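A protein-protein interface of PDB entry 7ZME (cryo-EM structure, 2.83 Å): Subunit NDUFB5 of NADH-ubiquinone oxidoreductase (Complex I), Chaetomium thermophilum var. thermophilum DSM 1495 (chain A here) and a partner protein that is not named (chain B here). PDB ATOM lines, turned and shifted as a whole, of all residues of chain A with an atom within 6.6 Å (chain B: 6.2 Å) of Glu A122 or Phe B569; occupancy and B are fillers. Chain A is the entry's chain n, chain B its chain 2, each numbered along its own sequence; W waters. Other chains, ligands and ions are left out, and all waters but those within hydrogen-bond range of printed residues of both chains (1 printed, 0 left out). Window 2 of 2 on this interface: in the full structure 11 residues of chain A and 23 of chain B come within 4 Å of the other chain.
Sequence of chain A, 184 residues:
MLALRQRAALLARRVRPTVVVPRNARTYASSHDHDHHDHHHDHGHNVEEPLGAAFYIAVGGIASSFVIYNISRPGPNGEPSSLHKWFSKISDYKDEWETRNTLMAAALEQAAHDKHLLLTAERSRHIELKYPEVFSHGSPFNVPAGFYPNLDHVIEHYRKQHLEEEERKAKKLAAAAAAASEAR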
ATOM      1  N   LEU A 117      11.571  -4.704 -35.365  1.00  0.00           N
ATOM      2  CA  LEU A 117      10.486  -3.824 -34.878  1.00  0.00           C
ATOM      3  C   LEU A 117      10.806  -3.328 -33.461  1.00  0.00           C
ATOM      4  O   LEU A 117      10.501  -2.161 -33.171  1.00  0.00           O
ATOM      5  CB  LEU A 117       9.192  -4.639 -34.928  1.00  0.00           C
ATOM      6  CG  LEU A 117       7.914  -3.889 -34.569  1.00  0.00           C
ATOM      7  CD1 LEU A 117       7.477  -3.002 -35.721  1.00  0.00           C
ATOM      8  CD2 LEU A 117       6.814  -4.867 -34.204  1.00  0.00           C
ATOM      9  N   LEU A 118      11.385  -4.182 -32.613  1.00  0.00           N
ATOM     10  CA  LEU A 118      11.709  -3.814 -31.212  1.00  0.00           C
ATOM     11  C   LEU A 118      12.926  -2.873 -31.126  1.00  0.00           C
ATOM     12  O   LEU A 118      12.811  -1.882 -30.392  1.00  0.00           O
ATOM     13  CB  LEU A 118      11.904  -5.087 -30.383  1.00  0.00           C
ATOM     14  CG  LEU A 118      10.653  -5.923 -30.119  1.00  0.00           C
ATOM     15  CD1 LEU A 118      11.027  -7.348 -29.749  1.00  0.00           C
ATOM     16  CD2 LEU A 118       9.798  -5.300 -29.030  1.00  0.00           C
ATOM     17  N   LEU A 119      14.045  -3.154 -31.805  1.00  0.00           N
ATOM     18  CA  LEU A 119      15.202  -2.277 -31.662  1.00  0.00           C
ATOM     19  C   LEU A 119      15.059  -0.975 -32.435  1.00  0.00           C
ATOM     20  O   LEU A 119      15.731   0.002 -32.098  1.00  0.00           O
ATOM     21  CB  LEU A 119      16.486  -2.995 -32.080  1.00  0.00           C
ATOM     22  CG  LEU A 119      17.109  -3.987 -31.093  1.00  0.00           C
ATOM     23  CD1 LEU A 119      16.314  -5.270 -30.942  1.00  0.00           C
ATOM     24  CD2 LEU A 119      18.532  -4.295 -31.523  1.00  0.00           C
ATOM     25  N   THR A 120      14.207  -0.934 -33.453  1.00  0.00           N
ATOM     26  CA  THR A 120      13.965   0.287 -34.204  1.00  0.00           C
ATOM     27  C   THR A 120      12.766   1.059 -33.682  1.00  0.00           C
ATOM     28  O   THR A 120      12.345   2.028 -34.318  1.00  0.00           O
ATOM     29  CB  THR A 120      13.771  -0.025 -35.686  1.00  0.00           C
ATOM     30  OG1 THR A 120      12.654  -0.906 -35.845  1.00  0.00           O
ATOM     31  CG2 THR A 120      15.013  -0.678 -36.264  1.00  0.00           C
ATOM     32  N   ALA A 121      12.205   0.646 -32.547  1.00  0.00           N
ATOM     33  CA  ALA A 121      11.057   1.340 -31.982  1.00  0.00           C
ATOM     34  C   ALA A 121      11.414   2.782 -31.662  1.00  0.00           C
ATOM     35  O   ALA A 121      12.499   3.074 -31.158  1.00  0.00           O
ATOM     36  CB  ALA A 121      10.569   0.624 -30.723  1.00  0.00           C
ATOM     37  N   GLU A 122      10.494   3.686 -31.977  1.00  0.00           N
ATOM     38  CA  GLU A 122      10.748   5.110 -31.809  1.00  0.00           C
ATOM     39  C   GLU A 122      10.916   5.453 -30.336  1.00  0.00           C
ATOM     40  O   GLU A 122      10.161   4.978 -29.483  1.00  0.00           O
ATOM     41  CB  GLU A 122       9.607   5.920 -32.418  1.00  0.00           C
ATOM     42  CG  GLU A 122       9.031   5.308 -33.684  1.00  0.00           C
ATOM     43  CD  GLU A 122       8.046   6.224 -34.382  1.00  0.00           C
ATOM     44  OE1 GLU A 122       7.441   7.078 -33.701  1.00  0.00           O
ATOM     45  OE2 GLU A 122       7.875   6.087 -35.611  1.00  0.00           O
ATOM     46  N   ARG A 123      11.916   6.273 -30.040  1.00  0.00           N
ATOM     47  CA  ARG A 123      12.139   6.739 -28.680  1.00  0.00           C
ATOM     48  C   ARG A 123      11.209   7.901 -28.370  1.00  0.00           C
ATOM     49  O   ARG A 123      11.103   8.855 -29.146  1.00  0.00           O
ATOM     50  CB  ARG A 123      13.593   7.166 -28.497  1.00  0.00           C
ATOM     51  CG  ARG A 123      13.867   7.911 -27.212  1.00  0.00           C
ATOM     52  CD  ARG A 123      15.135   8.717 -27.327  1.00  0.00           C
ATOM     53  NE  ARG A 123      15.656   9.111 -26.024  1.00  0.00           N
ATOM     54  CZ  ARG A 123      16.817   8.701 -25.530  1.00  0.00           C
ATOM     55  NH1 ARG A 123      17.580   7.878 -26.229  1.00  0.00           N
ATOM     56  NH2 ARG A 123      17.212   9.112 -24.338  1.00  0.00           N
ATOM     57  N   SER A 124      10.531   7.813 -27.231  1.00  0.00           N
ATOM     58  CA  SER A 124       9.600   8.859 -26.841  1.00  0.00           C
ATOM     59  C   SER A 124      10.347  10.111 -26.407  1.00  0.00           C
ATOM     60  O   SER A 124      11.337  10.046 -25.675  1.00  0.00           O
ATOM     61  CB  SER A 124       8.701   8.376 -25.708  1.00  0.00           C
ATOM     62  OG  SER A 124       7.825   9.405 -25.282  1.00  0.00           O
ATOM     63  N   LYS B  49       6.739   3.914 -16.512  1.00  0.00           N
ATOM     64  CA  LYS B  49       8.060   4.521 -16.530  1.00  0.00           C
ATOM     65  C   LYS B  49       8.479   5.048 -15.168  1.00  0.00           C
ATOM     66  O   LYS B  49       9.646   5.408 -14.991  1.00  0.00           O
ATOM     67  CB  LYS B  49       8.114   5.667 -17.539  1.00  0.00           C
ATOM     68  CG  LYS B  49       8.202   5.237 -18.977  1.00  0.00           C
ATOM     69  CD  LYS B  49       8.716   6.380 -19.824  1.00  0.00           C
ATOM     70  CE  LYS B  49       8.799   5.983 -21.270  1.00  0.00           C
ATOM     71  NZ  LYS B  49       7.440   5.858 -21.838  1.00  0.00           N
ATOM     72  N   TYR B 296      18.908   8.941 -20.085  1.00  0.00           N
ATOM     73  CA  TYR B 296      17.779   8.829 -21.042  1.00  0.00           C
ATOM     74  C   TYR B 296      16.936  10.102 -21.095  1.00  0.00           C
ATOM     75  O   TYR B 296      16.693  10.599 -22.202  1.00  0.00           O
ATOM     76  CB  TYR B 296      16.837   7.693 -20.643  1.00  0.00           C
ATOM     77  CG  TYR B 296      15.640   7.530 -21.546  1.00  0.00           C
ATOM     78  CD1 TYR B 296      15.722   6.772 -22.701  1.00  0.00           C
ATOM     79  CD2 TYR B 296      14.430   8.139 -21.259  1.00  0.00           C
ATOM     80  CE1 TYR B 296      14.640   6.632 -23.550  1.00  0.00           C
ATOM     81  CE2 TYR B 296      13.339   8.010 -22.100  1.00  0.00           C
ATOM     82  CZ  TYR B 296      13.444   7.251 -23.250  1.00  0.00           C
ATOM     83  OH  TYR B 296      12.377   7.106 -24.084  1.00  0.00           O
ATOM     84  N   SER B 358      22.791   6.041 -26.299  1.00  0.00           N
ATOM     85  CA  SER B 358      21.490   5.863 -25.606  1.00  0.00           C
ATOM     86  C   SER B 358      20.522   5.244 -26.601  1.00  0.00           C
ATOM     87  O   SER B 358      19.824   5.993 -27.299  1.00  0.00           O
ATOM     88  CB  SER B 358      20.978   7.140 -24.996  1.00  0.00           C
ATOM     89  OG  SER B 358      19.934   6.870 -24.068  1.00  0.00           O
ATOM     90  N   SER B 359      20.490   3.919 -26.633  1.00  0.00           N
ATOM     91  CA  SER B 359      19.671   3.218 -27.636  1.00  0.00           C
ATOM     92  C   SER B 359      19.018   2.016 -26.967  1.00  0.00           C
ATOM     93  O   SER B 359      19.505   1.608 -25.920  1.00  0.00           O
ATOM     94  CB  SER B 359      20.512   2.844 -28.818  1.00  0.00           C
ATOM     95  OG  SER B 359      21.303   1.699 -28.560  1.00  0.00           O
ATOM     96  N   ILE B 360      17.922   1.528 -27.526  1.00  0.00           N
ATOM     97  CA  ILE B 360      17.265   0.312 -26.982  1.00  0.00           C
ATOM     98  C   ILE B 360      18.319  -0.788 -26.883  1.00  0.00           C
ATOM     99  O   ILE B 360      18.426  -1.398 -25.817  1.00  0.00           O
ATOM    100  CB  ILE B 360      16.049  -0.072 -27.853  1.00  0.00           C
ATOM    101  CG1 ILE B 360      14.939   0.974 -27.769  1.00  0.00           C
ATOM    102  CG2 ILE B 360      15.545  -1.467 -27.525  1.00  0.00           C
ATOM    103  CD1 ILE B 360      14.006   0.966 -28.949  1.00  0.00           C
ATOM    104  N   SER B 362      21.663  -0.579 -26.820  1.00  0.00           N
ATOM    105  CA  SER B 362      22.700  -0.189 -25.827  1.00  0.00           C
ATOM    106  C   SER B 362      22.183  -0.310 -24.394  1.00  0.00           C
ATOM    107  O   SER B 362      23.014  -0.508 -23.508  1.00  0.00           O
ATOM    108  CB  SER B 362      23.198   1.192 -26.092  1.00  0.00           C
ATOM    109  OG  SER B 362      22.515   2.144 -25.297  1.00  0.00           O
ATOM    110  N   THR B 363      20.876  -0.199 -24.178  1.00  0.00           N
ATOM    111  CA  THR B 363      20.305  -0.182 -22.814  1.00  0.00           C
ATOM    112  C   THR B 363      20.127  -1.644 -22.432  1.00  0.00           C
ATOM    113  O   THR B 363      20.371  -1.972 -21.265  1.00  0.00           O
ATOM    114  CB  THR B 363      19.096   0.764 -22.727  1.00  0.00           C
ATOM    115  OG1 THR B 363      19.510   2.031 -23.236  1.00  0.00           O
ATOM    116  CG2 THR B 363      18.573   0.943 -21.320  1.00  0.00           C
ATOM    117  N   LEU B 564      12.357  -4.420 -19.969  1.00  0.00           N
ATOM    118  CA  LEU B 564      12.610  -3.244 -19.113  1.00  0.00           C
ATOM    119  C   LEU B 564      12.951  -2.072 -20.019  1.00  0.00           C
ATOM    120  O   LEU B 564      12.477  -0.966 -19.745  1.00  0.00           O
ATOM    121  CB  LEU B 564      13.768  -3.581 -18.177  1.00  0.00           C
ATOM    122  CG  LEU B 564      13.459  -3.571 -16.684  1.00  0.00           C
ATOM    123  CD1 LEU B 564      11.999  -3.892 -16.429  1.00  0.00           C
ATOM    124  CD2 LEU B 564      14.364  -4.545 -15.950  1.00  0.00           C
ATOM    125  N   VAL B 565      13.745  -2.325 -21.054  1.00  0.00           N
ATOM    126  CA  VAL B 565      14.190  -1.249 -21.981  1.00  0.00           C
ATOM    127  C   VAL B 565      13.027  -0.808 -22.862  1.00  0.00           C
ATOM    128  O   VAL B 565      12.928   0.387 -23.128  1.00  0.00           O
ATOM    129  CB  VAL B 565      15.408  -1.719 -22.791  1.00  0.00           C
ATOM    130  CG1 VAL B 565      15.805  -0.728 -23.870  1.00  0.00           C
ATOM    131  CG2 VAL B 565      16.577  -2.003 -21.866  1.00  0.00           C
ATOM    132  N   GLN B 566      12.161  -1.732 -23.253  1.00  0.00           N
ATOM    133  CA  GLN B 566      10.997  -1.341 -24.043  1.00  0.00           C
ATOM    134  C   GLN B 566      10.095  -0.402 -23.256  1.00  0.00           C
ATOM    135  O   GLN B 566       9.544   0.548 -23.816  1.00  0.00           O
ATOM    136  CB  GLN B 566      10.216  -2.572 -24.506  1.00  0.00           C
ATOM    137  CG  GLN B 566      10.875  -3.342 -25.645  1.00  0.00           C
ATOM    138  CD  GLN B 566      10.997  -2.535 -26.916  1.00  0.00           C
ATOM    139  OE1 GLN B 566      10.005  -2.048 -27.454  1.00  0.00           O
ATOM    140  NE2 GLN B 566      12.215  -2.378 -27.399  1.00  0.00           N
ATOM    141  N   ILE B 567       9.935  -0.652 -21.956  1.00  0.00           N
ATOM    142  CA  ILE B 567       9.132   0.232 -21.114  1.00  0.00           C
ATOM    143  C   ILE B 567       9.780   1.608 -21.013  1.00  0.00           C
ATOM    144  O   ILE B 567       9.105   2.639 -21.102  1.00  0.00           O
ATOM    145  CB  ILE B 567       8.916  -0.396 -19.726  1.00  0.00           C
ATOM    146  CG1 ILE B 567       8.113  -1.692 -19.849  1.00  0.00           C
ATOM    147  CG2 ILE B 567       8.230   0.585 -18.788  1.00  0.00           C
ATOM    148  CD1 ILE B 567       8.156  -2.559 -18.618  1.00  0.00           C
ATOM    149  N   LEU B 568      11.100   1.644 -20.825  1.00  0.00           N
ATOM    150  CA  LEU B 568      11.797   2.918 -20.674  1.00  0.00           C
ATOM    151  C   LEU B 568      11.725   3.763 -21.941  1.00  0.00           C
ATOM    152  O   LEU B 568      11.741   4.995 -21.863  1.00  0.00           O
ATOM    153  CB  LEU B 568      13.253   2.672 -20.278  1.00  0.00           C
ATOM    154  CG  LEU B 568      14.212   3.869 -20.256  1.00  0.00           C
ATOM    155  CD1 LEU B 568      13.939   4.791 -19.082  1.00  0.00           C
ATOM    156  CD2 LEU B 568      15.654   3.405 -20.251  1.00  0.00           C
ATOM    157  N   PHE B 569      11.652   3.129 -23.108  1.00  0.00           N
ATOM    158  CA  PHE B 569      11.611   3.836 -24.380  1.00  0.00           C
ATOM    159  C   PHE B 569      10.206   3.992 -24.943  1.00  0.00           C
ATOM    160  O   PHE B 569      10.044   4.626 -25.989  1.00  0.00           O
ATOM    161  CB  PHE B 569      12.485   3.116 -25.412  1.00  0.00           C
ATOM    162  CG  PHE B 569      13.945   3.434 -25.305  1.00  0.00           C
ATOM    163  CD1 PHE B 569      14.707   2.925 -24.271  1.00  0.00           C
ATOM    164  CD2 PHE B 569      14.562   4.223 -26.258  1.00  0.00           C
ATOM    165  CE1 PHE B 569      16.054   3.213 -24.180  1.00  0.00           C
ATOM    166  CE2 PHE B 569      15.906   4.510 -26.170  1.00  0.00           C
ATOM    167  CZ  PHE B 569      16.651   4.006 -25.129  1.00  0.00           C
ATOM    168  N   SER B 570       9.189   3.446 -24.283  1.00  0.00           N
ATOM    169  CA  SER B 570       7.850   3.391 -24.845  1.00  0.00           C
ATOM    170  C   SER B 570       7.116   4.717 -24.663  1.00  0.00           C
ATOM    171  O   SER B 570       7.683   5.722 -24.231  1.00  0.00           O
ATOM    172  CB  SER B 570       7.054   2.255 -24.209  1.00  0.00           C
ATOM    173  OG  SER B 570       7.493   1.001 -24.694  1.00  0.00           O
ATOM    174  N   ALA B 571       5.827   4.707 -25.000  1.00  0.00           N
ATOM    175  CA  ALA B 571       4.936   5.855 -24.845  1.00  0.00           C
ATOM    176  C   ALA B 571       5.523   7.132 -25.434  1.00  0.00           C
ATOM    177  O   ALA B 571       5.578   8.166 -24.768  1.00  0.00           O
ATOM    178  CB  ALA B 571       4.592   6.062 -23.377  1.00  0.00           C
HETATM  179  O   HOH W   1      18.378   0.306 -30.634  1.00  0.00           O
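Among the printed residues, merely in contact across the chains: Ser A124 with Ser B570 (3.2 Å), Ala A121 with Ile B360 (3.4 Å), Leu A118 with Ile B360 (3.4 Å), Ser A124 with Tyr B296 (3.5 Å), Glu A122 with Phe B569 (3.5 Å), Leu A119 with Ile B360 (3.7 Å) and Arg A123 with Phe B569 (3.8 Å).
NZ of Lys B49 sits at hydrogen-bond distance from O of Ser B570, 2.4 Å away.
O of Leu B568 lies within hydrogen-bond range of OH of Tyr B296, at 3.1 Å.
OG of Ser A124 lies within hydrogen-bond range of O of Ala B571 (2.6 Å).
The backbone carbonyl oxygen (O) of Phe B569 is in hydrogen-bond range of the backbone NH (N) of Ser A124 (3.5 Å).
The backbone carbonyl oxygen (O) of Leu A118 is in hydrogen-bond range of the side-chain amide nitrogen (NE2) of Gln B566, 3.1 Å away.
O of Tyr B296 sits at hydrogen-bond distance from NH2 of Arg A123, 2.7 Å away.
NH1 of Arg A123 sits at hydrogen-bond distance from O of Ser B358 (3.1 Å).
Printed residues of chain A that touch a printed residue of chain B: Leu A118, Leu A119, Ala A121, Glu A122, Arg A123 and Ser A124.
Hydrophobic or aromatic side chains of chain B within 4 Å of the printed part of chain A: Tyr B296, Ile B360 and Phe B569.
Among the printed residues, no Asp or Glu carboxylate lies within 4 Å of a Lys or Arg side-chain nitrogen of the other chain.
Of the printed residues of chain B, Glu A122 touches Phe B569 (3.5 Å).
Of the printed residues of chain A, Ser B358 touches Arg A123 (3.1 Å).
Of the printed residues of chain A, Ile B360 touches Leu A118, Leu A119 and Ala A121.
Thr B363 touches none of the printed residues of chain A.
Leu B564 touches none of the printed residues of chain A.
Phe B569 touches just these residues of chain A: Glu A122, Arg A123 and Ser A124.
Printed residues of chain A within 4 Å of Ser B570: Ser A124.
The nearest residue of chain B that does not touch Glu A122 is Ile B360 (5.4 Å).
The nearest residue of chain A that does not touch Phe B569 is Ala A121 (5.4 Å).
The nearest printed residue of chain B that does not touch Leu A118 is Phe B569 (7.1 Å).
Water W1 bridges the backbone carbonyl oxygen of Leu A119 (3.0 Å) and the backbone NH of Ile B360 (3.4 Å).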
